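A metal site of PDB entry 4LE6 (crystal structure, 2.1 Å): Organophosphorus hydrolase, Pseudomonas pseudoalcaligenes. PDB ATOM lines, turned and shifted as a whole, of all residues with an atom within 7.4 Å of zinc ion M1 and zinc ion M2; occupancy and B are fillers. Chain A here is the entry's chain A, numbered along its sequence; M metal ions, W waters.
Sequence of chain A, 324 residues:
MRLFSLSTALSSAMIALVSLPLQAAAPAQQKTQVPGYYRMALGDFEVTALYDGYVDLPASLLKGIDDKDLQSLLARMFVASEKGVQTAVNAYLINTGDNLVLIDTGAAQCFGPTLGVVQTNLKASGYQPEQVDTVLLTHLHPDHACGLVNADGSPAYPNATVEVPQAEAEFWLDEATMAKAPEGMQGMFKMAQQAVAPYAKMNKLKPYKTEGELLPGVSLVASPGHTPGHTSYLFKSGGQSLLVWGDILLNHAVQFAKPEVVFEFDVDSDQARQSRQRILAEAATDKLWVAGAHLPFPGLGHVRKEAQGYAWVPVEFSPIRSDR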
ATOM      1  N   ALA A  88      31.321   1.479   1.848  1.00  0.00           N
ATOM      2  CA  ALA A  88      30.709   1.286   0.539  1.00  0.00           C
ATOM      3  C   ALA A  88      29.350   1.943   0.524  1.00  0.00           C
ATOM      4  O   ALA A  88      28.702   2.086   1.572  1.00  0.00           O
ATOM      5  CB  ALA A  88      30.553  -0.197   0.268  1.00  0.00           C
ATOM      6  N   VAL A  89      28.926   2.344  -0.666  1.00  0.00           N
ATOM      7  CA  VAL A  89      27.569   2.835  -0.900  1.00  0.00           C
ATOM      8  C   VAL A  89      27.025   2.028  -2.074  1.00  0.00           C
ATOM      9  O   VAL A  89      27.580   2.070  -3.172  1.00  0.00           O
ATOM     10  CB  VAL A  89      27.580   4.329  -1.240  1.00  0.00           C
ATOM     11  CG1 VAL A  89      26.178   4.821  -1.580  1.00  0.00           C
ATOM     12  CG2 VAL A  89      28.165   5.135  -0.095  1.00  0.00           C
ATOM     13  N   ASP A 104      17.480   3.000  -4.439  1.00  0.00           N
ATOM     14  CA  ASP A 104      18.522   3.987  -4.185  1.00  0.00           C
ATOM     15  C   ASP A 104      19.350   4.248  -5.425  1.00  0.00           C
ATOM     16  O   ASP A 104      19.266   3.503  -6.395  1.00  0.00           O
ATOM     17  CB  ASP A 104      19.340   3.622  -2.958  1.00  0.00           C
ATOM     18  CG  ASP A 104      18.536   3.735  -1.674  1.00  0.00           C
ATOM     19  OD1 ASP A 104      17.469   4.398  -1.717  1.00  0.00           O
ATOM     20  OD2 ASP A 104      18.953   3.195  -0.621  1.00  0.00           O
ATOM     21  N   PHE A 111      29.041  13.964  -2.597  1.00  0.00           N
ATOM     22  CA  PHE A 111      30.088  13.709  -1.609  1.00  0.00           C
ATOM     23  C   PHE A 111      31.456  13.545  -2.270  1.00  0.00           C
ATOM     24  O   PHE A 111      32.356  12.915  -1.698  1.00  0.00           O
ATOM     25  CB  PHE A 111      29.732  12.448  -0.801  1.00  0.00           C
ATOM     26  CG  PHE A 111      28.726  12.675   0.291  1.00  0.00           C
ATOM     27  CD1 PHE A 111      28.711  13.869   0.999  1.00  0.00           C
ATOM     28  CD2 PHE A 111      27.805  11.701   0.622  1.00  0.00           C
ATOM     29  CE1 PHE A 111      27.789  14.083   1.995  1.00  0.00           C
ATOM     30  CE2 PHE A 111      26.882  11.909   1.638  1.00  0.00           C
ATOM     31  CZ  PHE A 111      26.877  13.107   2.316  1.00  0.00           C
ATOM     32  N   THR A 138      15.087   4.348  -0.156  1.00  0.00           N
ATOM     33  CA  THR A 138      14.949   3.923   1.237  1.00  0.00           C
ATOM     34  C   THR A 138      14.782   5.153   2.118  1.00  0.00           C
ATOM     35  O   THR A 138      14.030   5.129   3.089  1.00  0.00           O
ATOM     36  CB  THR A 138      16.128   3.060   1.735  1.00  0.00           C
ATOM     37  OG1 THR A 138      17.357   3.779   1.566  1.00  0.00           O
ATOM     38  CG2 THR A 138      16.185   1.789   0.942  1.00  0.00           C
ATOM     39  N   HIS A 139      15.473   6.234   1.769  1.00  0.00           N
ATOM     40  CA  HIS A 139      15.397   7.508   2.479  1.00  0.00           C
ATOM     41  C   HIS A 139      16.068   8.576   1.633  1.00  0.00           C
ATOM     42  O   HIS A 139      16.640   8.280   0.597  1.00  0.00           O
ATOM     43  CB  HIS A 139      16.022   7.433   3.895  1.00  0.00           C
ATOM     44  CG  HIS A 139      17.482   7.087   3.915  1.00  0.00           C
ATOM     45  ND1 HIS A 139      17.991   5.950   3.338  1.00  0.00           N
ATOM     46  CD2 HIS A 139      18.531   7.685   4.540  1.00  0.00           C
ATOM     47  CE1 HIS A 139      19.298   5.878   3.564  1.00  0.00           C
ATOM     48  NE2 HIS A 139      19.651   6.929   4.284  1.00  0.00           N
ATOM     49  N   LEU A 140      16.008   9.828   2.095  1.00  0.00           N
ATOM     50  CA  LEU A 140      16.376  10.966   1.248  1.00  0.00           C
ATOM     51  C   LEU A 140      17.794  11.481   1.453  1.00  0.00           C
ATOM     52  O   LEU A 140      18.169  12.551   0.942  1.00  0.00           O
ATOM     53  CB  LEU A 140      15.381  12.115   1.476  1.00  0.00           C
ATOM     54  CG  LEU A 140      13.946  11.794   1.069  1.00  0.00           C
ATOM     55  CD1 LEU A 140      13.031  13.019   1.260  1.00  0.00           C
ATOM     56  CD2 LEU A 140      13.883  11.271  -0.386  1.00  0.00           C
ATOM     57  N   HIS A 141      18.607  10.713   2.156  1.00  0.00           N
ATOM     58  CA  HIS A 141      19.987  11.107   2.363  1.00  0.00           C
ATOM     59  C   HIS A 141      20.690  11.238   1.004  1.00  0.00           C
ATOM     60  O   HIS A 141      20.347  10.531   0.057  1.00  0.00           O
ATOM     61  CB  HIS A 141      20.716  10.086   3.246  1.00  0.00           C
ATOM     62  CG  HIS A 141      20.622  10.360   4.711  1.00  0.00           C
ATOM     63  ND1 HIS A 141      20.971   9.415   5.666  1.00  0.00           N
ATOM     64  CD2 HIS A 141      20.262  11.477   5.393  1.00  0.00           C
ATOM     65  CE1 HIS A 141      20.810   9.930   6.870  1.00  0.00           C
ATOM     66  NE2 HIS A 141      20.384  11.179   6.730  1.00  0.00           N
ATOM     67  N   PRO A 142      21.674  12.148   0.907  1.00  0.00           N
ATOM     68  CA  PRO A 142      22.404  12.416  -0.334  1.00  0.00           C
ATOM     69  C   PRO A 142      22.939  11.149  -0.993  1.00  0.00           C
ATOM     70  O   PRO A 142      22.800  11.005  -2.218  1.00  0.00           O
ATOM     71  CB  PRO A 142      23.576  13.279   0.116  1.00  0.00           C
ATOM     72  CG  PRO A 142      23.176  13.860   1.404  1.00  0.00           C
ATOM     73  CD  PRO A 142      22.289  12.856   2.053  1.00  0.00           C
ATOM     74  N   ASP A 143      23.513  10.245  -0.205  1.00  0.00           N
ATOM     75  CA  ASP A 143      24.150   9.042  -0.756  1.00  0.00           C
ATOM     76  C   ASP A 143      23.142   8.007  -1.275  1.00  0.00           C
ATOM     77  O   ASP A 143      23.533   6.922  -1.746  1.00  0.00           O
ATOM     78  CB  ASP A 143      25.134   8.391   0.241  1.00  0.00           C
ATOM     79  CG  ASP A 143      24.512   8.103   1.616  1.00  0.00           C
ATOM     80  OD1 ASP A 143      23.860   9.006   2.168  1.00  0.00           O
ATOM     81  OD2 ASP A 143      24.687   6.978   2.152  1.00  0.00           O
ATOM     82  N   HIS A 144      21.859   8.349  -1.217  1.00  0.00           N
ATOM     83  CA  HIS A 144      20.783   7.517  -1.738  1.00  0.00           C
ATOM     84  C   HIS A 144      19.968   8.230  -2.804  1.00  0.00           C
ATOM     85  O   HIS A 144      19.470   7.596  -3.755  1.00  0.00           O
ATOM     86  CB  HIS A 144      19.883   7.059  -0.573  1.00  0.00           C
ATOM     87  CG  HIS A 144      20.640   6.303   0.467  1.00  0.00           C
ATOM     88  ND1 HIS A 144      20.654   4.928   0.519  1.00  0.00           N
ATOM     89  CD2 HIS A 144      21.463   6.725   1.458  1.00  0.00           C
ATOM     90  CE1 HIS A 144      21.447   4.529   1.494  1.00  0.00           C
ATOM     91  NE2 HIS A 144      21.944   5.603   2.090  1.00  0.00           N
ATOM     92  N   HIS A 226      16.767   5.992  11.419  1.00  0.00           N
ATOM     93  CA  HIS A 226      17.889   6.599  10.729  1.00  0.00           C
ATOM     94  C   HIS A 226      17.409   7.904  10.081  1.00  0.00           C
ATOM     95  O   HIS A 226      18.052   8.932  10.217  1.00  0.00           O
ATOM     96  CB  HIS A 226      18.452   5.633   9.694  1.00  0.00           C
ATOM     97  CG  HIS A 226      19.559   6.199   8.864  1.00  0.00           C
ATOM     98  ND1 HIS A 226      20.790   6.540   9.363  1.00  0.00           N
ATOM     99  CD2 HIS A 226      19.611   6.461   7.532  1.00  0.00           C
ATOM    100  CE1 HIS A 226      21.556   6.998   8.382  1.00  0.00           C
ATOM    101  NE2 HIS A 226      20.852   6.958   7.263  1.00  0.00           N
ATOM    102  N   THR A 227      16.261   7.843   9.389  1.00  0.00           N
ATOM    103  CA  THR A 227      15.447   9.036   9.154  1.00  0.00           C
ATOM    104  C   THR A 227      14.009   8.698   9.550  1.00  0.00           C
ATOM    105  O   THR A 227      13.634   7.527   9.621  1.00  0.00           O
ATOM    106  CB  THR A 227      15.445   9.492   7.682  1.00  0.00           C
ATOM    107  OG1 THR A 227      14.832   8.482   6.872  1.00  0.00           O
ATOM    108  CG2 THR A 227      16.845   9.780   7.176  1.00  0.00           C
ATOM    109  N   HIS A 230      12.428   6.477   7.119  1.00  0.00           N
ATOM    110  CA  HIS A 230      13.324   5.475   6.577  1.00  0.00           C
ATOM    111  C   HIS A 230      12.562   4.178   6.300  1.00  0.00           C
ATOM    112  O   HIS A 230      11.836   3.692   7.159  1.00  0.00           O
ATOM    113  CB  HIS A 230      14.478   5.197   7.530  1.00  0.00           C
ATOM    114  CG  HIS A 230      15.447   4.234   6.962  1.00  0.00           C
ATOM    115  ND1 HIS A 230      15.307   2.868   7.096  1.00  0.00           N
ATOM    116  CD2 HIS A 230      16.545   4.430   6.194  1.00  0.00           C
ATOM    117  CE1 HIS A 230      16.304   2.267   6.463  1.00  0.00           C
ATOM    118  NE2 HIS A 230      17.061   3.191   5.911  1.00  0.00           N
ATOM    119  N   GLY A 246      18.317  -0.606   3.146  1.00  0.00           N
ATOM    120  CA  GLY A 246      18.769   0.751   3.315  1.00  0.00           C
ATOM    121  C   GLY A 246      19.871   0.838   4.359  1.00  0.00           C
ATOM    122  O   GLY A 246      20.831   0.068   4.333  1.00  0.00           O
ATOM    123  N   ASP A 247      19.723   1.788   5.269  1.00  0.00           N
ATOM    124  CA  ASP A 247      20.724   2.114   6.258  1.00  0.00           C
ATOM    125  C   ASP A 247      20.413   1.567   7.658  1.00  0.00           C
ATOM    126  O   ASP A 247      20.682   2.222   8.670  1.00  0.00           O
ATOM    127  CB  ASP A 247      20.907   3.639   6.291  1.00  0.00           C
ATOM    128  CG  ASP A 247      21.702   4.159   5.110  1.00  0.00           C
ATOM    129  OD1 ASP A 247      21.861   3.406   4.126  1.00  0.00           O
ATOM    130  OD2 ASP A 247      22.155   5.321   5.155  1.00  0.00           O
ATOM    131  N   LEU A 249      22.106  -0.535   9.089  1.00  0.00           N
ATOM    132  CA  LEU A 249      23.354  -0.362   9.778  1.00  0.00           C
ATOM    133  C   LEU A 249      24.402   0.119   8.804  1.00  0.00           C
ATOM    134  O   LEU A 249      24.267  -0.017   7.582  1.00  0.00           O
ATOM    135  CB  LEU A 249      23.801  -1.621  10.523  1.00  0.00           C
ATOM    136  CG  LEU A 249      24.053  -2.917   9.771  1.00  0.00           C
ATOM    137  CD1 LEU A 249      25.528  -3.012   9.336  1.00  0.00           C
ATOM    138  CD2 LEU A 249      23.687  -4.082  10.661  1.00  0.00           C
ATOM    139  N   LEU A 250      25.421   0.716   9.375  1.00  0.00           N
ATOM    140  CA  LEU A 250      26.439   1.437   8.654  1.00  0.00           C
ATOM    141  C   LEU A 250      27.788   0.751   8.700  1.00  0.00           C
ATOM    142  O   LEU A 250      28.639   1.010   7.859  1.00  0.00           O
ATOM    143  CB  LEU A 250      26.578   2.820   9.290  1.00  0.00           C
ATOM    144  CG  LEU A 250      26.709   3.967   8.301  1.00  0.00           C
ATOM    145  CD1 LEU A 250      25.342   4.618   8.065  1.00  0.00           C
ATOM    146  CD2 LEU A 250      27.714   4.942   8.864  1.00  0.00           C
ATOM    147  N   PHE A 263      24.763   5.431  15.101  1.00  0.00           N
ATOM    148  CA  PHE A 263      25.476   6.328  14.203  1.00  0.00           C
ATOM    149  C   PHE A 263      25.094   7.783  14.507  1.00  0.00           C
ATOM    150  O   PHE A 263      23.910   8.098  14.666  1.00  0.00           O
ATOM    151  CB  PHE A 263      25.115   5.946  12.770  1.00  0.00           C
ATOM    152  CG  PHE A 263      25.832   6.729  11.710  1.00  0.00           C
ATOM    153  CD1 PHE A 263      27.204   6.843  11.704  1.00  0.00           C
ATOM    154  CD2 PHE A 263      25.115   7.317  10.682  1.00  0.00           C
ATOM    155  CE1 PHE A 263      27.850   7.560  10.705  1.00  0.00           C
ATOM    156  CE2 PHE A 263      25.752   8.017   9.678  1.00  0.00           C
ATOM    157  CZ  PHE A 263      27.110   8.142   9.695  1.00  0.00           C
ATOM    158  N   PHE A 265      24.672  10.301  12.825  1.00  0.00           N
ATOM    159  CA  PHE A 265      23.757  10.923  11.873  1.00  0.00           C
ATOM    160  C   PHE A 265      22.464  10.129  11.628  1.00  0.00           C
ATOM    161  O   PHE A 265      21.707  10.411  10.692  1.00  0.00           O
ATOM    162  CB  PHE A 265      24.493  11.218  10.578  1.00  0.00           C
ATOM    163  CG  PHE A 265      25.558  12.274  10.728  1.00  0.00           C
ATOM    164  CD1 PHE A 265      25.274  13.501  11.311  1.00  0.00           C
ATOM    165  CD2 PHE A 265      26.850  12.033  10.314  1.00  0.00           C
ATOM    166  CE1 PHE A 265      26.260  14.466  11.471  1.00  0.00           C
ATOM    167  CE2 PHE A 265      27.832  12.993  10.463  1.00  0.00           C
ATOM    168  CZ  PHE A 265      27.530  14.207  11.040  1.00  0.00           C
ATOM    169  N   ASP A 266      22.197   9.143  12.495  1.00  0.00           N
ATOM    170  CA  ASP A 266      20.830   8.684  12.677  1.00  0.00           C
ATOM    171  C   ASP A 266      20.037   9.897  13.204  1.00  0.00           C
ATOM    172  O   ASP A 266      20.459  10.531  14.173  1.00  0.00           O
ATOM    173  CB  ASP A 266      20.752   7.547  13.692  1.00  0.00           C
ATOM    174  CG  ASP A 266      21.363   6.260  13.187  1.00  0.00           C
ATOM    175  OD1 ASP A 266      21.324   5.999  11.972  1.00  0.00           O
ATOM    176  OD2 ASP A 266      21.875   5.491  14.025  1.00  0.00           O
ATOM    177  N   ALA A 293      22.791  -1.109   1.838  1.00  0.00           N
ATOM    178  CA  ALA A 293      23.409   0.032   1.180  1.00  0.00           C
ATOM    179  C   ALA A 293      24.841   0.274   1.614  1.00  0.00           C
ATOM    180  O   ALA A 293      25.646   0.809   0.837  1.00  0.00           O
ATOM    181  CB  ALA A 293      22.586   1.273   1.422  1.00  0.00           C
ATOM    182  N   HIS A 294      25.180  -0.083   2.847  1.00  0.00           N
ATOM    183  CA  HIS A 294      26.530   0.179   3.357  1.00  0.00           C
ATOM    184  C   HIS A 294      27.268  -1.063   3.825  1.00  0.00           C
ATOM    185  O   HIS A 294      28.272  -0.982   4.549  1.00  0.00           O
ATOM    186  CB  HIS A 294      26.472   1.239   4.462  1.00  0.00           C
ATOM    187  CG  HIS A 294      25.910   2.539   3.998  1.00  0.00           C
ATOM    188  ND1 HIS A 294      26.450   3.240   2.938  1.00  0.00           N
ATOM    189  CD2 HIS A 294      24.825   3.245   4.387  1.00  0.00           C
ATOM    190  CE1 HIS A 294      25.737   4.316   2.712  1.00  0.00           C
ATOM    191  NE2 HIS A 294      24.730   4.348   3.575  1.00  0.00           N
HETATM  192 ZN    ZN M   1      21.433   7.425   5.450  1.00  0.00          ZN
HETATM  193 ZN    ZN M   2      23.400   5.904   3.518  1.00  0.00          ZN
HETATM  194  O   HOH W   1      24.073   7.777   6.687  1.00  0.00           O
HETATM  195  O   HOH W   2      23.184   7.569   4.240  1.00  0.00           O
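A ring nitrogen (ND1) of His 226 lies within hydrogen-bond range of the side-chain carboxylate (OD1) of Asp 266 (2.7 Å). The backbone carbonyl oxygen (O) of Ala 88 sits at hydrogen-bond distance from a ring nitrogen (ND1) of His 294 (2.9 Å). A ring nitrogen (ND1) of His 144 sits at hydrogen-bond distance from the side-chain carboxylate of Asp 104. N of Asp 247 lies within hydrogen-bond range of NE2 of His 230, 3.1 Å away. The side-chain hydroxyl (OG1) of Thr 138 lies within hydrogen-bond range of a ring nitrogen (ND1) of His 139 (2.9 Å).
Within 4 Å of zinc ion M1: His 139, His 141, His 144, His 226 and Asp 247. The nearest printed residue that does not touch zinc ion M1 is Asp 143 (4.4 Å).
Along chain A the residues within 4 Å of zinc ion M2 span positions 139 to 294.
Zinc ion M1 is bound by a ring nitrogen (NE2) of His 226 (2.0 Å), a ring nitrogen (ND1) of His 141 (2.1 Å), water W2 (2.1 Å), a ring nitrogen (NE2) of His 139 (2.2 Å) and the side-chain carboxylate of Asp 247 (2.2 Å). Zinc ion M1 has five donor atoms within binding distance.
Zinc ion M2 is bound by water W2, a ring nitrogen (NE2) of His 294, a ring nitrogen (NE2) of His 144, the side-chain carboxylate (OD2) of Asp 247 and the side-chain carboxylate (OD2) of Asp 143.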
